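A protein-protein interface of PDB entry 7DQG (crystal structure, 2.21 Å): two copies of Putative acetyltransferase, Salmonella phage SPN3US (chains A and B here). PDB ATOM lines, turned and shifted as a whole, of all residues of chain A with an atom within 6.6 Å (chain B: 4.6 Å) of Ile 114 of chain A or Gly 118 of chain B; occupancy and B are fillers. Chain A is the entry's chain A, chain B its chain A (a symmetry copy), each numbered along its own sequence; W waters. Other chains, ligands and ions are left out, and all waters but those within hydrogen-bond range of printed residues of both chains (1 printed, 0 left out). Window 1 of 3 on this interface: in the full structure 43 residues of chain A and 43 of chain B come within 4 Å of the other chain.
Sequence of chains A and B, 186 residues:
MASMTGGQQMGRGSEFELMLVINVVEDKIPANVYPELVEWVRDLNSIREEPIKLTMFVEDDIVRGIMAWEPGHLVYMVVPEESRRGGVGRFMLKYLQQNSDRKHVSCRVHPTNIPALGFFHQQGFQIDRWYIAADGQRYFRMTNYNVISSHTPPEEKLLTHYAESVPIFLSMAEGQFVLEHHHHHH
Water W1 lies within hydrogen-bond range of the side-chain amide oxygen (OE1) of Gln 126 of chain B (2.6 Å) and the backbone carbonyl oxygen (O) of Pro 111 of chain A (2.8 Å).
Among the printed residues, merely in contact across the chains: Thr 112 of chain A with His 121 of chain B (3.8 Å), Thr 112 of chain A with Gln 126 of chain B (3.9 Å), Ile 114 of chain A with Leu 117 of chain B (3.6 Å), Ile 114 of chain A with Gly 118 of chain B (3.7 Å), Ile 114 of chain A with His 121 of chain B (3.6 Å), Ile 114 of chain A with Met 142 of chain B (3.8 Å), Pro 115 of chain A with His 121 of chain B (3.7 Å), Leu 117 of chain A with Ile 114 of chain B (3.6 Å) and Gly 118 of chain A with Ile 114 of chain B (3.7 Å).
Ile 114 of chain A touches Leu 117 of chain B, and with the chains exchanged Leu 117 of chain A touches Ile 114 of chain B. Ile 114 of chain A touches Gly 118 of chain B, and with the chains exchanged Gly 118 of chain A touches Ile 114 of chain B. 6 positions are printed for both chains. Of the 9 pairs that touch across the chains among the printed residues, 4 have their exchanged pair printed and touching as well.
Of the printed residues of chain B, Thr 112 of chain A touches His 121 and Gln 126. Of the printed residues of chain B, Gly 118 of chain A touches Ile 114 (3.7 Å). Phe 119 of chain A touches none of the printed residues of chain B. Gly 118 of chain B touches just one residue of chain A: Ile 114 (3.7 Å). Phe 119 of chain B touches none of the printed residues of chain A. Of the printed residues of chain A, Gln 126 of chain B touches Thr 112. Of the printed residues of chain A, Met 142 of chain B touches Ile 114. The nearest residue of chain B that does not touch Ile 114 of chain A is Gln 126 of chain B (4.3 Å).
A ring nitrogen (ND1) of His 110 of chain A lies within hydrogen-bond range of the side-chain hydroxyl (OG1) of Thr 112 of chain A, at 2.6 Å.
Of the 11 printed residues of chain A, 5 touch a printed residue of chain B. Hydrophobic or aromatic side chains of chain A within 4 Å of the printed part of chain B: Ile 114 and Pro 115. Of the 11 printed residues of chain B, 6 touch a printed residue of chain A. Among the printed residues, no Asp or Glu carboxylate lies within 4 Å of a Lys or Arg side-chain nitrogen of the other chain.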
ATOM      1  N   VAL A 109     -26.973 -36.838  -2.351  1.00  0.00           N
ATOM      2  CA  VAL A 109     -27.705 -35.587  -2.188  1.00  0.00           C
ATOM      3  C   VAL A 109     -27.053 -34.523  -3.060  1.00  0.00           C
ATOM      4  O   VAL A 109     -25.829 -34.363  -3.040  1.00  0.00           O
ATOM      5  CB  VAL A 109     -27.738 -35.114  -0.719  1.00  0.00           C
ATOM      6  CG1 VAL A 109     -28.652 -33.905  -0.574  1.00  0.00           C
ATOM      7  CG2 VAL A 109     -28.179 -36.237   0.215  1.00  0.00           C
ATOM      8  N   HIS A 110     -27.869 -33.789  -3.815  1.00  0.00           N
ATOM      9  CA  HIS A 110     -27.347 -32.678  -4.597  1.00  0.00           C
ATOM     10  C   HIS A 110     -26.885 -31.556  -3.667  1.00  0.00           C
ATOM     11  O   HIS A 110     -27.502 -31.323  -2.622  1.00  0.00           O
ATOM     12  CB  HIS A 110     -28.407 -32.153  -5.566  1.00  0.00           C
ATOM     13  CG  HIS A 110     -27.853 -31.297  -6.662  1.00  0.00           C
ATOM     14  ND1 HIS A 110     -27.694 -29.933  -6.535  1.00  0.00           N
ATOM     15  CD2 HIS A 110     -27.409 -31.613  -7.903  1.00  0.00           C
ATOM     16  CE1 HIS A 110     -27.181 -29.445  -7.650  1.00  0.00           C
ATOM     17  NE2 HIS A 110     -27.000 -30.444  -8.496  1.00  0.00           N
ATOM     18  N   PRO A 111     -25.799 -30.856  -4.008  1.00  0.00           N
ATOM     19  CA  PRO A 111     -25.313 -29.782  -3.125  1.00  0.00           C
ATOM     20  C   PRO A 111     -26.301 -28.644  -2.933  1.00  0.00           C
ATOM     21  O   PRO A 111     -26.170 -27.894  -1.957  1.00  0.00           O
ATOM     22  CB  PRO A 111     -24.036 -29.301  -3.829  1.00  0.00           C
ATOM     23  CG  PRO A 111     -23.586 -30.481  -4.627  1.00  0.00           C
ATOM     24  CD  PRO A 111     -24.848 -31.147  -5.095  1.00  0.00           C
ATOM     25  N   THR A 112     -27.283 -28.483  -3.824  1.00  0.00           N
ATOM     26  CA  THR A 112     -28.297 -27.453  -3.626  1.00  0.00           C
ATOM     27  C   THR A 112     -29.385 -27.883  -2.652  1.00  0.00           C
ATOM     28  O   THR A 112     -30.110 -27.024  -2.136  1.00  0.00           O
ATOM     29  CB  THR A 112     -28.939 -27.066  -4.961  1.00  0.00           C
ATOM     30  OG1 THR A 112     -29.460 -28.237  -5.600  1.00  0.00           O
ATOM     31  CG2 THR A 112     -27.917 -26.398  -5.878  1.00  0.00           C
ATOM     32  N   ASN A 113     -29.515 -29.184  -2.387  1.00  0.00           N
ATOM     33  CA  ASN A 113     -30.518 -29.696  -1.454  1.00  0.00           C
ATOM     34  C   ASN A 113     -29.986 -29.636  -0.020  1.00  0.00           C
ATOM     35  O   ASN A 113     -29.850 -30.641   0.681  1.00  0.00           O
ATOM     36  CB  ASN A 113     -30.925 -31.113  -1.839  1.00  0.00           C
ATOM     37  CG  ASN A 113     -32.238 -31.533  -1.205  1.00  0.00           C
ATOM     38  OD1 ASN A 113     -32.795 -30.819  -0.369  1.00  0.00           O
ATOM     39  ND2 ASN A 113     -32.737 -32.701  -1.597  1.00  0.00           N
ATOM     40  N   ILE A 114     -29.684 -28.409   0.409  1.00  0.00           N
ATOM     41  CA  ILE A 114     -29.156 -28.205   1.760  1.00  0.00           C
ATOM     42  C   ILE A 114     -30.164 -28.600   2.835  1.00  0.00           C
ATOM     43  O   ILE A 114     -29.745 -29.139   3.871  1.00  0.00           O
ATOM     44  CB  ILE A 114     -28.626 -26.775   1.907  1.00  0.00           C
ATOM     45  CG1 ILE A 114     -27.354 -26.616   1.065  1.00  0.00           C
ATOM     46  CG2 ILE A 114     -28.343 -26.432   3.364  1.00  0.00           C
ATOM     47  CD1 ILE A 114     -26.824 -25.201   0.973  1.00  0.00           C
ATOM     48  N   PRO A 115     -31.481 -28.382   2.675  1.00  0.00           N
ATOM     49  CA  PRO A 115     -32.425 -28.943   3.664  1.00  0.00           C
ATOM     50  C   PRO A 115     -32.263 -30.439   3.894  1.00  0.00           C
ATOM     51  O   PRO A 115     -32.319 -30.890   5.045  1.00  0.00           O
ATOM     52  CB  PRO A 115     -33.793 -28.610   3.057  1.00  0.00           C
ATOM     53  CG  PRO A 115     -33.559 -27.345   2.316  1.00  0.00           C
ATOM     54  CD  PRO A 115     -32.158 -27.439   1.762  1.00  0.00           C
ATOM     55  N   ALA A 116     -32.067 -31.225   2.832  1.00  0.00           N
ATOM     56  CA  ALA A 116     -31.847 -32.656   3.012  1.00  0.00           C
ATOM     57  C   ALA A 116     -30.534 -32.925   3.736  1.00  0.00           C
ATOM     58  O   ALA A 116     -30.452 -33.843   4.562  1.00  0.00           O
ATOM     59  CB  ALA A 116     -31.872 -33.373   1.664  1.00  0.00           C
ATOM     60  N   LEU A 117     -29.496 -32.135   3.440  1.00  0.00           N
ATOM     61  CA  LEU A 117     -28.240 -32.258   4.173  1.00  0.00           C
ATOM     62  C   LEU A 117     -28.462 -32.066   5.668  1.00  0.00           C
ATOM     63  O   LEU A 117     -27.900 -32.803   6.487  1.00  0.00           O
ATOM     64  CB  LEU A 117     -27.218 -31.246   3.655  1.00  0.00           C
ATOM     65  CG  LEU A 117     -26.783 -31.333   2.189  1.00  0.00           C
ATOM     66  CD1 LEU A 117     -25.748 -30.262   1.884  1.00  0.00           C
ATOM     67  CD2 LEU A 117     -26.237 -32.710   1.859  1.00  0.00           C
ATOM     68  N   GLY A 118     -29.279 -31.080   6.041  1.00  0.00           N
ATOM     69  CA  GLY A 118     -29.575 -30.872   7.449  1.00  0.00           C
ATOM     70  C   GLY A 118     -30.301 -32.048   8.072  1.00  0.00           C
ATOM     71  O   GLY A 118     -30.011 -32.438   9.206  1.00  0.00           O
ATOM     72  N   PHE A 119     -31.249 -32.635   7.336  1.00  0.00           N
ATOM     73  CA  PHE A 119     -31.961 -33.807   7.835  1.00  0.00           C
ATOM     74  C   PHE A 119     -30.997 -34.956   8.106  1.00  0.00           C
ATOM     75  O   PHE A 119     -30.942 -35.490   9.219  1.00  0.00           O
ATOM     76  CB  PHE A 119     -33.044 -34.236   6.843  1.00  0.00           C
ATOM     77  CG  PHE A 119     -33.585 -35.618   7.100  1.00  0.00           C
ATOM     78  CD1 PHE A 119     -34.418 -35.861   8.183  1.00  0.00           C
ATOM     79  CD2 PHE A 119     -33.257 -36.674   6.264  1.00  0.00           C
ATOM     80  CE1 PHE A 119     -34.915 -37.131   8.426  1.00  0.00           C
ATOM     81  CE2 PHE A 119     -33.750 -37.947   6.501  1.00  0.00           C
ATOM     82  CZ  PHE A 119     -34.581 -38.176   7.584  1.00  0.00           C
ATOM     83  N   ILE B 114     -22.820 -28.446   8.743  1.00  0.00           N
ATOM     84  CA  ILE B 114     -24.080 -28.446   7.997  1.00  0.00           C
ATOM     85  C   ILE B 114     -25.100 -27.485   8.595  1.00  0.00           C
ATOM     86  O   ILE B 114     -25.845 -26.855   7.826  1.00  0.00           O
ATOM     87  CB  ILE B 114     -24.599 -29.880   7.840  1.00  0.00           C
ATOM     88  CG1 ILE B 114     -23.684 -30.650   6.880  1.00  0.00           C
ATOM     89  CG2 ILE B 114     -26.036 -29.901   7.336  1.00  0.00           C
ATOM     90  CD1 ILE B 114     -23.975 -32.131   6.774  1.00  0.00           C
ATOM     91  N   PRO B 115     -25.202 -27.308   9.924  1.00  0.00           N
ATOM     92  CA  PRO B 115     -26.081 -26.237  10.440  1.00  0.00           C
ATOM     93  C   PRO B 115     -25.800 -24.865   9.844  1.00  0.00           C
ATOM     94  O   PRO B 115     -26.744 -24.134   9.518  1.00  0.00           O
ATOM     95  CB  PRO B 115     -25.806 -26.265  11.948  1.00  0.00           C
ATOM     96  CG  PRO B 115     -25.480 -27.687  12.227  1.00  0.00           C
ATOM     97  CD  PRO B 115     -24.737 -28.191  11.013  1.00  0.00           C
ATOM     98  N   ALA B 116     -24.527 -24.490   9.694  1.00  0.00           N
ATOM     99  CA  ALA B 116     -24.211 -23.208   9.072  1.00  0.00           C
ATOM    100  C   ALA B 116     -24.624 -23.190   7.606  1.00  0.00           C
ATOM    101  O   ALA B 116     -25.096 -22.163   7.102  1.00  0.00           O
ATOM    102  CB  ALA B 116     -22.721 -22.900   9.212  1.00  0.00           C
ATOM    103  N   LEU B 117     -24.454 -24.317   6.906  1.00  0.00           N
ATOM    104  CA  LEU B 117     -24.931 -24.411   5.530  1.00  0.00           C
ATOM    105  C   LEU B 117     -26.424 -24.125   5.450  1.00  0.00           C
ATOM    106  O   LEU B 117     -26.881 -23.417   4.545  1.00  0.00           O
ATOM    107  CB  LEU B 117     -24.625 -25.794   4.953  1.00  0.00           C
ATOM    108  CG  LEU B 117     -23.163 -26.237   4.854  1.00  0.00           C
ATOM    109  CD1 LEU B 117     -23.074 -27.622   4.232  1.00  0.00           C
ATOM    110  CD2 LEU B 117     -22.340 -25.243   4.056  1.00  0.00           C
ATOM    111  N   GLY B 118     -27.200 -24.666   6.392  1.00  0.00           N
ATOM    112  CA  GLY B 118     -28.627 -24.393   6.405  1.00  0.00           C
ATOM    113  C   GLY B 118     -28.938 -22.928   6.636  1.00  0.00           C
ATOM    114  O   GLY B 118     -29.839 -22.368   6.007  1.00  0.00           O
ATOM    115  N   PHE B 119     -28.192 -22.285   7.538  1.00  0.00           N
ATOM    116  CA  PHE B 119     -28.387 -20.859   7.786  1.00  0.00           C
ATOM    117  C   PHE B 119     -28.142 -20.047   6.520  1.00  0.00           C
ATOM    118  O   PHE B 119     -29.010 -19.287   6.078  1.00  0.00           O
ATOM    119  CB  PHE B 119     -27.468 -20.385   8.915  1.00  0.00           C
ATOM    120  CG  PHE B 119     -27.345 -18.886   9.003  1.00  0.00           C
ATOM    121  CD1 PHE B 119     -28.398 -18.116   9.475  1.00  0.00           C
ATOM    122  CD2 PHE B 119     -26.180 -18.246   8.607  1.00  0.00           C
ATOM    123  CE1 PHE B 119     -28.291 -16.737   9.554  1.00  0.00           C
ATOM    124  CE2 PHE B 119     -26.066 -16.868   8.683  1.00  0.00           C
ATOM    125  CZ  PHE B 119     -27.124 -16.112   9.158  1.00  0.00           C
ATOM    126  N   PHE B 120     -26.961 -20.206   5.914  1.00  0.00           N
ATOM    127  CA  PHE B 120     -26.620 -19.410   4.738  1.00  0.00           C
ATOM    128  C   PHE B 120     -27.559 -19.706   3.574  1.00  0.00           C
ATOM    129  O   PHE B 120     -27.943 -18.796   2.830  1.00  0.00           O
ATOM    130  CB  PHE B 120     -25.165 -19.661   4.336  1.00  0.00           C
ATOM    131  CG  PHE B 120     -24.163 -19.109   5.312  1.00  0.00           C
ATOM    132  CD1 PHE B 120     -24.099 -17.748   5.568  1.00  0.00           C
ATOM    133  CD2 PHE B 120     -23.283 -19.951   5.974  1.00  0.00           C
ATOM    134  CE1 PHE B 120     -23.179 -17.238   6.466  1.00  0.00           C
ATOM    135  CE2 PHE B 120     -22.361 -19.447   6.874  1.00  0.00           C
ATOM    136  CZ  PHE B 120     -22.310 -18.089   7.121  1.00  0.00           C
ATOM    137  N   HIS B 121     -27.940 -20.976   3.403  1.00  0.00           N
ATOM    138  CA  HIS B 121     -28.883 -21.336   2.349  1.00  0.00           C
ATOM    139  C   HIS B 121     -30.203 -20.595   2.514  1.00  0.00           C
ATOM    140  O   HIS B 121     -30.775 -20.103   1.534  1.00  0.00           O
ATOM    141  CB  HIS B 121     -29.114 -22.847   2.352  1.00  0.00           C
ATOM    142  CG  HIS B 121     -30.214 -23.296   1.442  1.00  0.00           C
ATOM    143  ND1 HIS B 121     -30.056 -23.401   0.076  1.00  0.00           N
ATOM    144  CD2 HIS B 121     -31.488 -23.678   1.703  1.00  0.00           C
ATOM    145  CE1 HIS B 121     -31.185 -23.823  -0.466  1.00  0.00           C
ATOM    146  NE2 HIS B 121     -32.069 -23.998   0.500  1.00  0.00           N
ATOM    147  N   GLN B 122     -30.699 -20.500   3.749  1.00  0.00           N
ATOM    148  CA  GLN B 122     -31.934 -19.771   4.006  1.00  0.00           C
ATOM    149  C   GLN B 122     -31.791 -18.282   3.722  1.00  0.00           C
ATOM    150  O   GLN B 122     -32.802 -17.603   3.512  1.00  0.00           O
ATOM    151  CB  GLN B 122     -32.377 -19.995   5.455  1.00  0.00           C
ATOM    152  CG  GLN B 122     -33.842 -19.681   5.719  1.00  0.00           C
ATOM    153  CD  GLN B 122     -34.787 -20.622   4.993  1.00  0.00           C
ATOM    154  OE1 GLN B 122     -34.412 -21.736   4.620  1.00  0.00           O
ATOM    155  NE2 GLN B 122     -36.021 -20.178   4.788  1.00  0.00           N
ATOM    156  N   GLN B 126     -25.505 -20.189  -1.871  1.00  0.00           N
ATOM    157  CA  GLN B 126     -25.337 -21.528  -2.413  1.00  0.00           C
ATOM    158  C   GLN B 126     -23.856 -21.876  -2.446  1.00  0.00           C
ATOM    159  O   GLN B 126     -22.998 -20.993  -2.520  1.00  0.00           O
ATOM    160  CB  GLN B 126     -25.927 -21.656  -3.830  1.00  0.00           C
ATOM    161  CG  GLN B 126     -27.442 -21.489  -3.917  1.00  0.00           C
ATOM    162  CD  GLN B 126     -28.205 -22.757  -3.562  1.00  0.00           C
ATOM    163  OE1 GLN B 126     -27.651 -23.691  -2.983  1.00  0.00           O
ATOM    164  NE2 GLN B 126     -29.486 -22.791  -3.912  1.00  0.00           N
ATOM    165  N   MET B 142     -19.454 -20.322  -0.179  1.00  0.00           N
ATOM    166  CA  MET B 142     -20.859 -19.996  -0.375  1.00  0.00           C
ATOM    167  C   MET B 142     -20.973 -18.520  -0.718  1.00  0.00           C
ATOM    168  O   MET B 142     -20.382 -17.673  -0.039  1.00  0.00           O
ATOM    169  CB  MET B 142     -21.689 -20.327   0.872  1.00  0.00           C
ATOM    170  CG  MET B 142     -21.861 -21.821   1.134  1.00  0.00           C
ATOM    171  SD  MET B 142     -23.120 -22.190   2.381  1.00  0.00           S
ATOM    172  CE  MET B 142     -24.618 -22.107   1.402  1.00  0.00           C
HETATM  173  O   HOH W   1     -25.618 -25.196  -2.584  1.00  0.00           O
